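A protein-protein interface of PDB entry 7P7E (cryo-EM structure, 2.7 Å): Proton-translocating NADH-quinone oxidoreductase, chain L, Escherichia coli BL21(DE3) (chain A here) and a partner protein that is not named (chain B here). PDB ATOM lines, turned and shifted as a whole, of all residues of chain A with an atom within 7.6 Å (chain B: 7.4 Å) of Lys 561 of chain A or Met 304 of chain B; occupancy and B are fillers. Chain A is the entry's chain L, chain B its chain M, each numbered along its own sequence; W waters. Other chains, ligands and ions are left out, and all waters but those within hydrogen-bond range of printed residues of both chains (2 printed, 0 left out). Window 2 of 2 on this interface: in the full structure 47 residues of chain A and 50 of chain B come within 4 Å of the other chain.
Among the printed residues, pairs that only touch across the chains: Ile 556 of chain A with Trp 303 of chain B (3.5 Å), Ala 557 of chain A with Trp 303 of chain B (3.96 Å), Ala 557 of chain A with Phe 306 of chain B (3.7 Å), Ala 557 of chain A with Ala 307 of chain B (3.7 Å), Leu 560 of chain A with Ala 307 of chain B (3.9 Å), Lys 561 of chain A with Met 304 of chain B (3.99 Å), Lys 561 of chain A with Ala 307 of chain B (3.8 Å), Asp 563 of chain A with Met 304 of chain B (3.8 Å), Leu 565 of chain A with His 241 of chain B (3.9 Å) and Leu 565 of chain A with Tyr 300 of chain B (3.5 Å).
SD of Met 304 of chain B is in hydrogen-bond range of OH of Tyr 300 of chain B (3.7 Å). NE2 of Gln 308 of chain B is in hydrogen-bond range of O of Met 304 of chain B (3.0 Å). NH2 of Arg 442 of chain B is in hydrogen-bond range of O of Phe 306 of chain B. The backbone carbonyl oxygen (O) of Trp 558 of chain A lies close to the side-chain amino group (NZ) of Lys 561 of chain A, at 3.4 Å.
Of the printed residues of chain B, Lys 561 of chain A touches Met 304 and Ala 307. Of the printed residues of chain A, Met 304 of chain B touches Leu 560, Lys 561 and Asp 563. Of the printed residues of chain A, Tyr 300 of chain B touches Asp 563 (2.3 Å), Pro 564 (3.3 Å) and Leu 565 (3.5 Å). Of the printed residues of chain A, Ala 307 of chain B touches Ala 557 (3.7 Å), Leu 560 (3.9 Å) and Lys 561 (3.8 Å). Of the printed residues of chain B, Ile 556 of chain A touches Trp 303 (3.5 Å). Printed residues of chain B within 4 Å of Ala 557 of chain A: Trp 303 (3.96 Å), Phe 306 (3.7 Å) and Ala 307 (3.7 Å). Of the printed residues of chain B, Leu 565 of chain A touches His 241 and Tyr 300. Phe 299 of chain B touches none of the printed residues of chain A. Gly 301 of chain B touches none of the printed residues of chain A. The nearest printed residue of chain A that does not touch Met 304 of chain B is Arg 562 of chain A (4.4 Å).
Of the 12 printed residues of chain A, 7 touch a printed residue of chain B. Hydrophobic or aromatic side chains of chain A within 4 Å of the printed part of chain B: Ile 556, Ala 557, Pro 564 and Leu 565. Of the 22 printed residues of chain B, 7 touch a printed residue of chain A. Hydrophobic or aromatic side chains of chain B that line the printed part of chain A: His 241, Tyr 300, Trp 303, Met 304, Phe 306, Ala 307 and Tyr 317. Among the printed residues, 15 pairs touch across the chains.
A ring nitrogen (NE2) of His 241 of chain B lies within hydrogen-bond range of the side-chain carboxylate of Asp 563 of chain A, 3.1 Å away. The side-chain hydroxyl (OH) of Tyr 317 of chain B lies within hydrogen-bond range of the side-chain carboxylate (OD2) of Asp 563 of chain A (2.5 Å). The backbone carbonyl oxygen of Leu 560 of chain A lies close to the side-chain sulfur of Met 304 of chain B, at 3.2 Å. The side-chain carboxylate of Asp 563 of chain A lies close to the side-chain hydroxyl of Tyr 300 of chain B (2.3 Å). N of Pro 564 of chain A sits close to OH of Tyr 300 of chain B (3.4 Å).
Water W1 lies within hydrogen-bond range of ND2 of Asn 566 of chain A, OD2 of Asp 563 of chain A and OH of Tyr 317 of chain B. Water W2 bridges O of Lys 561 of chain A (3.3 Å) and OE1 of Gln 308 of chain B (3.4 Å).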
ATOM      1  N   GLY A 555       0.747   4.175 -25.999  1.00  0.00           N
ATOM      2  CA  GLY A 555       0.074   5.353 -25.476  1.00  0.00           C
ATOM      3  C   GLY A 555      -1.306   5.052 -24.922  1.00  0.00           C
ATOM      4  O   GLY A 555      -1.664   5.525 -23.840  1.00  0.00           O
ATOM      5  N   ILE A 556      -2.092   4.251 -25.643  1.00  0.00           N
ATOM      6  CA  ILE A 556      -3.418   3.875 -25.159  1.00  0.00           C
ATOM      7  C   ILE A 556      -3.307   2.960 -23.942  1.00  0.00           C
ATOM      8  O   ILE A 556      -4.102   3.064 -23.001  1.00  0.00           O
ATOM      9  CB  ILE A 556      -4.239   3.239 -26.296  1.00  0.00           C
ATOM     10  CG1 ILE A 556      -4.482   4.264 -27.402  1.00  0.00           C
ATOM     11  CG2 ILE A 556      -5.586   2.747 -25.798  1.00  0.00           C
ATOM     12  CD1 ILE A 556      -5.014   3.665 -28.680  1.00  0.00           C
ATOM     13  N   ALA A 557      -2.308   2.071 -23.925  1.00  0.00           N
ATOM     14  CA  ALA A 557      -2.100   1.209 -22.764  1.00  0.00           C
ATOM     15  C   ALA A 557      -1.709   2.013 -21.529  1.00  0.00           C
ATOM     16  O   ALA A 557      -2.147   1.700 -20.416  1.00  0.00           O
ATOM     17  CB  ALA A 557      -1.040   0.153 -23.074  1.00  0.00           C
ATOM     18  N   TRP A 558      -0.881   3.046 -21.701  1.00  0.00           N
ATOM     19  CA  TRP A 558      -0.538   3.915 -20.581  1.00  0.00           C
ATOM     20  C   TRP A 558      -1.720   4.782 -20.161  1.00  0.00           C
ATOM     21  O   TRP A 558      -1.865   5.094 -18.974  1.00  0.00           O
ATOM     22  CB  TRP A 558       0.666   4.783 -20.947  1.00  0.00           C
ATOM     23  CG  TRP A 558       1.050   5.769 -19.892  1.00  0.00           C
ATOM     24  CD1 TRP A 558       1.889   5.558 -18.837  1.00  0.00           C
ATOM     25  CD2 TRP A 558       0.615   7.130 -19.793  1.00  0.00           C
ATOM     26  NE1 TRP A 558       2.000   6.702 -18.086  1.00  0.00           N
ATOM     27  CE2 TRP A 558       1.228   7.681 -18.651  1.00  0.00           C
ATOM     28  CE3 TRP A 558      -0.236   7.933 -20.557  1.00  0.00           C
ATOM     29  CZ2 TRP A 558       1.018   8.999 -18.256  1.00  0.00           C
ATOM     30  CZ3 TRP A 558      -0.444   9.241 -20.163  1.00  0.00           C
ATOM     31  CH2 TRP A 558       0.181   9.762 -19.023  1.00  0.00           C
ATOM     32  N   LEU A 559      -2.563   5.186 -21.112  1.00  0.00           N
ATOM     33  CA  LEU A 559      -3.765   5.940 -20.771  1.00  0.00           C
ATOM     34  C   LEU A 559      -4.765   5.062 -20.029  1.00  0.00           C
ATOM     35  O   LEU A 559      -5.542   5.562 -19.207  1.00  0.00           O
ATOM     36  CB  LEU A 559      -4.361   6.537 -22.057  1.00  0.00           C
ATOM     37  CG  LEU A 559      -5.536   7.521 -22.240  1.00  0.00           C
ATOM     38  CD1 LEU A 559      -5.651   7.845 -23.720  1.00  0.00           C
ATOM     39  CD2 LEU A 559      -6.902   7.050 -21.745  1.00  0.00           C
ATOM     40  N   LEU A 560      -4.733   3.755 -20.278  1.00  0.00           N
ATOM     41  CA  LEU A 560      -5.679   2.820 -19.686  1.00  0.00           C
ATOM     42  C   LEU A 560      -4.955   1.816 -18.802  1.00  0.00           C
ATOM     43  O   LEU A 560      -5.147   0.608 -18.952  1.00  0.00           O
ATOM     44  CB  LEU A 560      -6.468   2.080 -20.769  1.00  0.00           C
ATOM     45  CG  LEU A 560      -7.323   2.879 -21.753  1.00  0.00           C
ATOM     46  CD1 LEU A 560      -7.890   1.959 -22.820  1.00  0.00           C
ATOM     47  CD2 LEU A 560      -8.439   3.600 -21.031  1.00  0.00           C
ATOM     48  N   LYS A 561      -4.081   2.290 -17.918  1.00  0.00           N
ATOM     49  CA  LYS A 561      -3.434   1.414 -16.954  1.00  0.00           C
ATOM     50  C   LYS A 561      -4.072   1.474 -15.575  1.00  0.00           C
ATOM     51  O   LYS A 561      -3.712   0.669 -14.709  1.00  0.00           O
ATOM     52  CB  LYS A 561      -1.943   1.754 -16.836  1.00  0.00           C
ATOM     53  CG  LYS A 561      -1.670   3.164 -16.362  1.00  0.00           C
ATOM     54  CD  LYS A 561      -0.183   3.408 -16.177  1.00  0.00           C
ATOM     55  CE  LYS A 561       0.069   4.726 -15.466  1.00  0.00           C
ATOM     56  NZ  LYS A 561      -1.018   5.709 -15.732  1.00  0.00           N
ATOM     57  N   ARG A 562      -5.005   2.399 -15.350  1.00  0.00           N
ATOM     58  CA  ARG A 562      -5.642   2.560 -14.049  1.00  0.00           C
ATOM     59  C   ARG A 562      -7.141   2.289 -14.088  1.00  0.00           C
ATOM     60  O   ARG A 562      -7.839   2.628 -13.123  1.00  0.00           O
ATOM     61  CB  ARG A 562      -5.376   3.965 -13.500  1.00  0.00           C
ATOM     62  CG  ARG A 562      -3.907   4.239 -13.215  1.00  0.00           C
ATOM     63  CD  ARG A 562      -3.725   5.451 -12.318  1.00  0.00           C
ATOM     64  NE  ARG A 562      -2.316   5.729 -12.061  1.00  0.00           N
ATOM     65  CZ  ARG A 562      -1.624   6.699 -12.643  1.00  0.00           C
ATOM     66  NH1 ARG A 562      -2.183   7.516 -13.521  1.00  0.00           N
ATOM     67  NH2 ARG A 562      -0.340   6.853 -12.336  1.00  0.00           N
ATOM     68  N   ASP A 563      -7.650   1.697 -15.179  1.00  0.00           N
ATOM     69  CA  ASP A 563      -9.029   1.240 -15.350  1.00  0.00           C
ATOM     70  C   ASP A 563     -10.042   2.367 -15.161  1.00  0.00           C
ATOM     71  O   ASP A 563     -10.715   2.416 -14.124  1.00  0.00           O
ATOM     72  CB  ASP A 563      -9.325   0.089 -14.386  1.00  0.00           C
ATOM     73  CG  ASP A 563     -10.266  -0.940 -14.976  1.00  0.00           C
ATOM     74  OD1 ASP A 563     -10.947  -0.627 -15.970  1.00  0.00           O
ATOM     75  OD2 ASP A 563     -10.320  -2.069 -14.444  1.00  0.00           O
ATOM     76  N   PRO A 564     -10.156   3.300 -16.115  1.00  0.00           N
ATOM     77  CA  PRO A 564     -11.095   4.427 -15.944  1.00  0.00           C
ATOM     78  C   PRO A 564     -12.558   4.022 -15.843  1.00  0.00           C
ATOM     79  O   PRO A 564     -13.331   4.710 -15.160  1.00  0.00           O
ATOM     80  CB  PRO A 564     -10.840   5.284 -17.192  1.00  0.00           C
ATOM     81  CG  PRO A 564      -9.501   4.858 -17.689  1.00  0.00           C
ATOM     82  CD  PRO A 564      -9.413   3.404 -17.381  1.00  0.00           C
ATOM     83  N   LEU A 565     -12.966   2.939 -16.511  1.00  0.00           N
ATOM     84  CA  LEU A 565     -14.350   2.484 -16.413  1.00  0.00           C
ATOM     85  C   LEU A 565     -14.669   2.000 -15.005  1.00  0.00           C
ATOM     86  O   LEU A 565     -15.777   2.221 -14.497  1.00  0.00           O
ATOM     87  CB  LEU A 565     -14.609   1.382 -17.439  1.00  0.00           C
ATOM     88  CG  LEU A 565     -14.632   1.829 -18.901  1.00  0.00           C
ATOM     89  CD1 LEU A 565     -14.687   0.629 -19.834  1.00  0.00           C
ATOM     90  CD2 LEU A 565     -15.793   2.772 -19.166  1.00  0.00           C
ATOM     91  N   ASN A 566     -13.694   1.361 -14.353  1.00  0.00           N
ATOM     92  CA  ASN A 566     -13.849   0.961 -12.959  1.00  0.00           C
ATOM     93  C   ASN A 566     -14.025   2.173 -12.049  1.00  0.00           C
ATOM     94  O   ASN A 566     -14.848   2.148 -11.129  1.00  0.00           O
ATOM     95  CB  ASN A 566     -12.641   0.134 -12.527  1.00  0.00           C
ATOM     96  CG  ASN A 566     -12.850  -0.562 -11.203  1.00  0.00           C
ATOM     97  OD1 ASN A 566     -13.960  -0.610 -10.678  1.00  0.00           O
ATOM     98  ND2 ASN A 566     -11.775  -1.104 -10.650  1.00  0.00           N
ATOM     99  N   VAL B 238     -18.268  -4.889 -19.773  1.00  0.00           N
ATOM    100  CA  VAL B 238     -17.821  -3.537 -19.427  1.00  0.00           C
ATOM    101  C   VAL B 238     -19.028  -2.606 -19.402  1.00  0.00           C
ATOM    102  O   VAL B 238     -19.949  -2.768 -20.227  1.00  0.00           O
ATOM    103  CB  VAL B 238     -16.759  -3.044 -20.426  1.00  0.00           C
ATOM    104  CG1 VAL B 238     -15.412  -3.669 -20.112  1.00  0.00           C
ATOM    105  CG2 VAL B 238     -17.172  -3.372 -21.847  1.00  0.00           C
ATOM    106  N   HIS B 241     -17.265  -4.777 -15.073  1.00  0.00           N
ATOM    107  CA  HIS B 241     -16.209  -5.759 -14.886  1.00  0.00           C
ATOM    108  C   HIS B 241     -15.325  -5.471 -13.684  1.00  0.00           C
ATOM    109  O   HIS B 241     -14.503  -6.321 -13.330  1.00  0.00           O
ATOM    110  CB  HIS B 241     -15.314  -5.789 -16.121  1.00  0.00           C
ATOM    111  CG  HIS B 241     -14.482  -4.555 -16.264  1.00  0.00           C
ATOM    112  ND1 HIS B 241     -15.013  -3.345 -16.653  1.00  0.00           N
ATOM    113  CD2 HIS B 241     -13.169  -4.329 -16.024  1.00  0.00           C
ATOM    114  CE1 HIS B 241     -14.060  -2.432 -16.669  1.00  0.00           C
ATOM    115  NE2 HIS B 241     -12.931  -3.004 -16.292  1.00  0.00           N
ATOM    116  N   ILE B 298     -13.666  -6.857 -25.466  1.00  0.00           N
ATOM    117  CA  ILE B 298     -12.501  -7.533 -26.041  1.00  0.00           C
ATOM    118  C   ILE B 298     -11.286  -6.613 -26.035  1.00  0.00           C
ATOM    119  O   ILE B 298     -10.231  -6.942 -25.474  1.00  0.00           O
ATOM    120  CB  ILE B 298     -12.810  -8.015 -27.472  1.00  0.00           C
ATOM    121  CG1 ILE B 298     -13.783  -9.189 -27.470  1.00  0.00           C
ATOM    122  CG2 ILE B 298     -11.530  -8.399 -28.202  1.00  0.00           C
ATOM    123  CD1 ILE B 298     -14.255  -9.566 -28.847  1.00  0.00           C
ATOM    124  N   PHE B 299     -11.442  -5.416 -26.599  1.00  0.00           N
ATOM    125  CA  PHE B 299     -10.270  -4.560 -26.763  1.00  0.00           C
ATOM    126  C   PHE B 299      -9.854  -3.910 -25.451  1.00  0.00           C
ATOM    127  O   PHE B 299      -8.655  -3.753 -25.184  1.00  0.00           O
ATOM    128  CB  PHE B 299     -10.528  -3.518 -27.839  1.00  0.00           C
ATOM    129  CG  PHE B 299     -10.209  -4.010 -29.201  1.00  0.00           C
ATOM    130  CD1 PHE B 299      -8.907  -3.998 -29.665  1.00  0.00           C
ATOM    131  CD2 PHE B 299     -11.197  -4.543 -29.997  1.00  0.00           C
ATOM    132  CE1 PHE B 299      -8.607  -4.475 -30.919  1.00  0.00           C
ATOM    133  CE2 PHE B 299     -10.903  -5.021 -31.240  1.00  0.00           C
ATOM    134  CZ  PHE B 299      -9.609  -4.987 -31.709  1.00  0.00           C
ATOM    135  N   TYR B 300     -10.823  -3.533 -24.618  1.00  0.00           N
ATOM    136  CA  TYR B 300     -10.512  -2.954 -23.321  1.00  0.00           C
ATOM    137  C   TYR B 300      -9.848  -3.970 -22.407  1.00  0.00           C
ATOM    138  O   TYR B 300      -8.897  -3.633 -21.699  1.00  0.00           O
ATOM    139  CB  TYR B 300     -11.783  -2.404 -22.686  1.00  0.00           C
ATOM    140  CG  TYR B 300     -11.536  -1.626 -21.425  1.00  0.00           C
ATOM    141  CD1 TYR B 300     -11.033  -0.335 -21.474  1.00  0.00           C
ATOM    142  CD2 TYR B 300     -11.805  -2.181 -20.184  1.00  0.00           C
ATOM    143  CE1 TYR B 300     -10.808   0.381 -20.324  1.00  0.00           C
ATOM    144  CE2 TYR B 300     -11.584  -1.473 -19.029  1.00  0.00           C
ATOM    145  CZ  TYR B 300     -11.086  -0.193 -19.106  1.00  0.00           C
ATOM    146  OH  TYR B 300     -10.865   0.516 -17.957  1.00  0.00           O
ATOM    147  N   GLY B 301     -10.321  -5.220 -22.416  1.00  0.00           N
ATOM    148  CA  GLY B 301      -9.663  -6.254 -21.643  1.00  0.00           C
ATOM    149  C   GLY B 301      -8.266  -6.552 -22.145  1.00  0.00           C
ATOM    150  O   GLY B 301      -7.364  -6.821 -21.352  1.00  0.00           O
ATOM    151  N   ALA B 302      -8.059  -6.478 -23.465  1.00  0.00           N
ATOM    152  CA  ALA B 302      -6.716  -6.678 -24.004  1.00  0.00           C
ATOM    153  C   ALA B 302      -5.757  -5.572 -23.566  1.00  0.00           C
ATOM    154  O   ALA B 302      -4.646  -5.850 -23.093  1.00  0.00           O
ATOM    155  CB  ALA B 302      -6.773  -6.771 -25.527  1.00  0.00           C
ATOM    156  N   TRP B 303      -6.176  -4.312 -23.711  1.00  0.00           N
ATOM    157  CA  TRP B 303      -5.339  -3.188 -23.296  1.00  0.00           C
ATOM    158  C   TRP B 303      -5.103  -3.189 -21.792  1.00  0.00           C
ATOM    159  O   TRP B 303      -4.006  -2.854 -21.332  1.00  0.00           O
ATOM    160  CB  TRP B 303      -5.977  -1.871 -23.732  1.00  0.00           C
ATOM    161  CG  TRP B 303      -5.447  -1.334 -25.020  1.00  0.00           C
ATOM    162  CD1 TRP B 303      -4.138  -1.134 -25.348  1.00  0.00           C
ATOM    163  CD2 TRP B 303      -6.213  -0.922 -26.157  1.00  0.00           C
ATOM    164  NE1 TRP B 303      -4.043  -0.622 -26.618  1.00  0.00           N
ATOM    165  CE2 TRP B 303      -5.303  -0.484 -27.136  1.00  0.00           C
ATOM    166  CE3 TRP B 303      -7.581  -0.880 -26.439  1.00  0.00           C
ATOM    167  CZ2 TRP B 303      -5.715  -0.007 -28.378  1.00  0.00           C
ATOM    168  CZ3 TRP B 303      -7.988  -0.410 -27.671  1.00  0.00           C
ATOM    169  CH2 TRP B 303      -7.059   0.018 -28.627  1.00  0.00           C
ATOM    170  N   MET B 304      -6.127  -3.550 -21.015  1.00  0.00           N
ATOM    171  CA  MET B 304      -5.986  -3.679 -19.571  1.00  0.00           C
ATOM    172  C   MET B 304      -5.002  -4.778 -19.202  1.00  0.00           C
ATOM    173  O   MET B 304      -4.193  -4.609 -18.287  1.00  0.00           O
ATOM    174  CB  MET B 304      -7.354  -3.967 -18.952  1.00  0.00           C
ATOM    175  CG  MET B 304      -8.252  -2.786 -18.558  1.00  0.00           C
ATOM    176  SD  MET B 304      -7.622  -1.158 -18.088  1.00  0.00           S
ATOM    177  CE  MET B 304      -6.417  -1.513 -16.799  1.00  0.00           C
ATOM    178  N   ALA B 305      -5.065  -5.914 -19.900  1.00  0.00           N
ATOM    179  CA  ALA B 305      -4.157  -7.018 -19.622  1.00  0.00           C
ATOM    180  C   ALA B 305      -2.716  -6.648 -19.946  1.00  0.00           C
ATOM    181  O   ALA B 305      -1.799  -7.020 -19.207  1.00  0.00           O
ATOM    182  CB  ALA B 305      -4.585  -8.258 -20.405  1.00  0.00           C
ATOM    183  N   PHE B 306      -2.497  -5.910 -21.039  1.00  0.00           N
ATOM    184  CA  PHE B 306      -1.137  -5.504 -21.382  1.00  0.00           C
ATOM    185  C   PHE B 306      -0.550  -4.548 -20.350  1.00  0.00           C
ATOM    186  O   PHE B 306       0.660  -4.574 -20.102  1.00  0.00           O
ATOM    187  CB  PHE B 306      -1.108  -4.864 -22.772  1.00  0.00           C
ATOM    188  CG  PHE B 306       0.264  -4.435 -23.216  1.00  0.00           C
ATOM    189  CD1 PHE B 306       1.153  -5.355 -23.739  1.00  0.00           C
ATOM    190  CD2 PHE B 306       0.663  -3.111 -23.110  1.00  0.00           C
ATOM    191  CE1 PHE B 306       2.415  -4.966 -24.147  1.00  0.00           C
ATOM    192  CE2 PHE B 306       1.924  -2.718 -23.512  1.00  0.00           C
ATOM    193  CZ  PHE B 306       2.799  -3.646 -24.032  1.00  0.00           C
ATOM    194  N   ALA B 307      -1.382  -3.712 -19.731  1.00  0.00           N
ATOM    195  CA  ALA B 307      -0.895  -2.676 -18.830  1.00  0.00           C
ATOM    196  C   ALA B 307      -0.565  -3.182 -17.430  1.00  0.00           C
ATOM    197  O   ALA B 307       0.038  -2.435 -16.654  1.00  0.00           O
ATOM    198  CB  ALA B 307      -1.923  -1.549 -18.733  1.00  0.00           C
ATOM    199  N   GLN B 308      -0.936  -4.411 -17.086  1.00  0.00           N
ATOM    200  CA  GLN B 308      -0.742  -4.893 -15.726  1.00  0.00           C
ATOM    201  C   GLN B 308       0.719  -5.235 -15.454  1.00  0.00           C
ATOM    202  O   GLN B 308       1.467  -5.637 -16.348  1.00  0.00           O
ATOM    203  CB  GLN B 308      -1.603  -6.129 -15.460  1.00  0.00           C
ATOM    204  CG  GLN B 308      -3.097  -5.900 -15.562  1.00  0.00           C
ATOM    205  CD  GLN B 308      -3.569  -4.721 -14.742  1.00  0.00           C
ATOM    206  OE1 GLN B 308      -3.399  -4.690 -13.527  1.00  0.00           O
ATOM    207  NE2 GLN B 308      -4.169  -3.741 -15.406  1.00  0.00           N
ATOM    208  N   THR B 309       1.120  -5.056 -14.197  1.00  0.00           N
ATOM    209  CA  THR B 309       2.343  -5.645 -13.670  1.00  0.00           C
ATOM    210  C   THR B 309       2.065  -6.870 -12.812  1.00  0.00           C
ATOM    211  O   THR B 309       3.002  -7.591 -12.460  1.00  0.00           O
ATOM    212  CB  THR B 309       3.132  -4.617 -12.848  1.00  0.00           C
ATOM    213  OG1 THR B 309       2.376  -4.247 -11.688  1.00  0.00           O
ATOM    214  CG2 THR B 309       3.417  -3.379 -13.677  1.00  0.00           C
ATOM    215  N   ASP B 310       0.803  -7.111 -12.477  1.00  0.00           N
ATOM    216  CA  ASP B 310       0.364  -8.296 -11.754  1.00  0.00           C
ATOM    217  C   ASP B 310      -0.126  -9.330 -12.757  1.00  0.00           C
ATOM    218  O   ASP B 310      -0.865  -8.995 -13.686  1.00  0.00           O
ATOM    219  CB  ASP B 310      -0.747  -7.927 -10.764  1.00  0.00           C
ATOM    220  CG  ASP B 310      -0.915  -8.942  -9.648  1.00  0.00           C
ATOM    221  OD1 ASP B 310      -0.684 -10.143  -9.881  1.00  0.00           O
ATOM    222  OD2 ASP B 310      -1.286  -8.534  -8.531  1.00  0.00           O
ATOM    223  N   ARG B 313      -4.155 -10.090 -12.235  1.00  0.00           N
ATOM    224  CA  ARG B 313      -4.988  -9.066 -12.857  1.00  0.00           C
ATOM    225  C   ARG B 313      -4.973  -9.194 -14.375  1.00  0.00           C
ATOM    226  O   ARG B 313      -6.009  -9.016 -15.032  1.00  0.00           O
ATOM    227  CB  ARG B 313      -4.515  -7.681 -12.423  1.00  0.00           C
ATOM    228  CG  ARG B 313      -4.483  -7.497 -10.918  1.00  0.00           C
ATOM    229  CD  ARG B 313      -4.248  -6.049 -10.533  1.00  0.00           C
ATOM    230  NE  ARG B 313      -5.383  -5.200 -10.872  1.00  0.00           N
ATOM    231  CZ  ARG B 313      -6.442  -5.019 -10.097  1.00  0.00           C
ATOM    232  NH1 ARG B 313      -6.550  -5.615  -8.922  1.00  0.00           N
ATOM    233  NH2 ARG B 313      -7.418  -4.215 -10.510  1.00  0.00           N
ATOM    234  N   LEU B 314      -3.807  -9.524 -14.942  1.00  0.00           N
ATOM    235  CA  LEU B 314      -3.692  -9.758 -16.379  1.00  0.00           C
ATOM    236  C   LEU B 314      -4.621 -10.883 -16.826  1.00  0.00           C
ATOM    237  O   LEU B 314      -5.363 -10.733 -17.801  1.00  0.00           O
ATOM    238  CB  LEU B 314      -2.235 -10.074 -16.732  1.00  0.00           C
ATOM    239  CG  LEU B 314      -1.749 -10.256 -18.175  1.00  0.00           C
ATOM    240  CD1 LEU B 314      -0.331  -9.743 -18.302  1.00  0.00           C
ATOM    241  CD2 LEU B 314      -1.799 -11.713 -18.617  1.00  0.00           C
ATOM    242  N   TYR B 317      -8.224  -9.862 -16.844  1.00  0.00           N
ATOM    243  CA  TYR B 317      -8.591  -9.064 -18.009  1.00  0.00           C
ATOM    244  C   TYR B 317      -8.657  -9.905 -19.285  1.00  0.00           C
ATOM    245  O   TYR B 317      -9.454  -9.600 -20.188  1.00  0.00           O
ATOM    246  CB  TYR B 317      -7.626  -7.894 -18.144  1.00  0.00           C
ATOM    247  CG  TYR B 317      -7.899  -6.820 -17.117  1.00  0.00           C
ATOM    248  CD1 TYR B 317      -9.169  -6.281 -16.975  1.00  0.00           C
ATOM    249  CD2 TYR B 317      -6.892  -6.344 -16.293  1.00  0.00           C
ATOM    250  CE1 TYR B 317      -9.425  -5.299 -16.043  1.00  0.00           C
ATOM    251  CE2 TYR B 317      -7.140  -5.367 -15.354  1.00  0.00           C
ATOM    252  CZ  TYR B 317      -8.406  -4.847 -15.236  1.00  0.00           C
ATOM    253  OH  TYR B 317      -8.655  -3.870 -14.303  1.00  0.00           O
ATOM    254  N   THR B 318      -7.858 -10.975 -19.370  1.00  0.00           N
ATOM    255  CA  THR B 318      -8.033 -11.936 -20.463  1.00  0.00           C
ATOM    256  C   THR B 318      -9.413 -12.578 -20.412  1.00  0.00           C
ATOM    257  O   THR B 318     -10.044 -12.807 -21.455  1.00  0.00           O
ATOM    258  CB  THR B 318      -6.969 -13.033 -20.421  1.00  0.00           C
ATOM    259  OG1 THR B 318      -7.175 -13.863 -19.272  1.00  0.00           O
ATOM    260  CG2 THR B 318      -5.584 -12.458 -20.387  1.00  0.00           C
ATOM    261  N   VAL B 320     -12.057 -11.129 -19.243  1.00  0.00           N
ATOM    262  CA  VAL B 320     -12.966 -10.083 -19.726  1.00  0.00           C
ATOM    263  C   VAL B 320     -13.024 -10.066 -21.256  1.00  0.00           C
ATOM    264  O   VAL B 320     -14.109  -9.983 -21.852  1.00  0.00           O
ATOM    265  CB  VAL B 320     -12.542  -8.713 -19.160  1.00  0.00           C
ATOM    266  CG1 VAL B 320     -13.393  -7.600 -19.744  1.00  0.00           C
ATOM    267  CG2 VAL B 320     -12.636  -8.712 -17.646  1.00  0.00           C
ATOM    268  N   TYR B 435      -0.836  -9.497 -25.784  1.00  0.00           N
ATOM    269  CA  TYR B 435      -0.723  -9.523 -24.322  1.00  0.00           C
ATOM    270  C   TYR B 435      -0.186 -10.859 -23.809  1.00  0.00           C
ATOM    271  O   TYR B 435       0.509 -10.884 -22.784  1.00  0.00           O
ATOM    272  CB  TYR B 435      -2.044  -9.144 -23.615  1.00  0.00           C
ATOM    273  CG  TYR B 435      -3.311  -9.977 -23.805  1.00  0.00           C
ATOM    274  CD1 TYR B 435      -3.366 -11.332 -23.488  1.00  0.00           C
ATOM    275  CD2 TYR B 435      -4.484  -9.371 -24.213  1.00  0.00           C
ATOM    276  CE1 TYR B 435      -4.519 -12.060 -23.656  1.00  0.00           C
ATOM    277  CE2 TYR B 435      -5.655 -10.087 -24.352  1.00  0.00           C
ATOM    278  CZ  TYR B 435      -5.665 -11.432 -24.075  1.00  0.00           C
ATOM    279  OH  TYR B 435      -6.823 -12.154 -24.227  1.00  0.00           O
ATOM    280  N   ARG B 442       7.732 -10.851 -20.002  1.00  0.00           N
ATOM    281  CA  ARG B 442       7.978 -10.204 -18.718  1.00  0.00           C
ATOM    282  C   ARG B 442       8.276 -11.222 -17.626  1.00  0.00           C
ATOM    283  O   ARG B 442       9.127 -10.980 -16.765  1.00  0.00           O
ATOM    284  CB  ARG B 442       6.782  -9.343 -18.319  1.00  0.00           C
ATOM    285  CG  ARG B 442       6.632  -8.065 -19.110  1.00  0.00           C
ATOM    286  CD  ARG B 442       5.311  -7.408 -18.778  1.00  0.00           C
ATOM    287  NE  ARG B 442       4.817  -6.576 -19.864  1.00  0.00           N
ATOM    288  CZ  ARG B 442       3.562  -6.164 -19.971  1.00  0.00           C
ATOM    289  NH1 ARG B 442       2.649  -6.493 -19.073  1.00  0.00           N
ATOM    290  NH2 ARG B 442       3.214  -5.405 -21.004  1.00  0.00           N
HETATM  291  O   HOH W   1     -10.492  -2.782 -11.882  1.00  0.00           O
HETATM  292  O   HOH W   2      -4.803  -1.689 -12.751  1.00  0.00           O
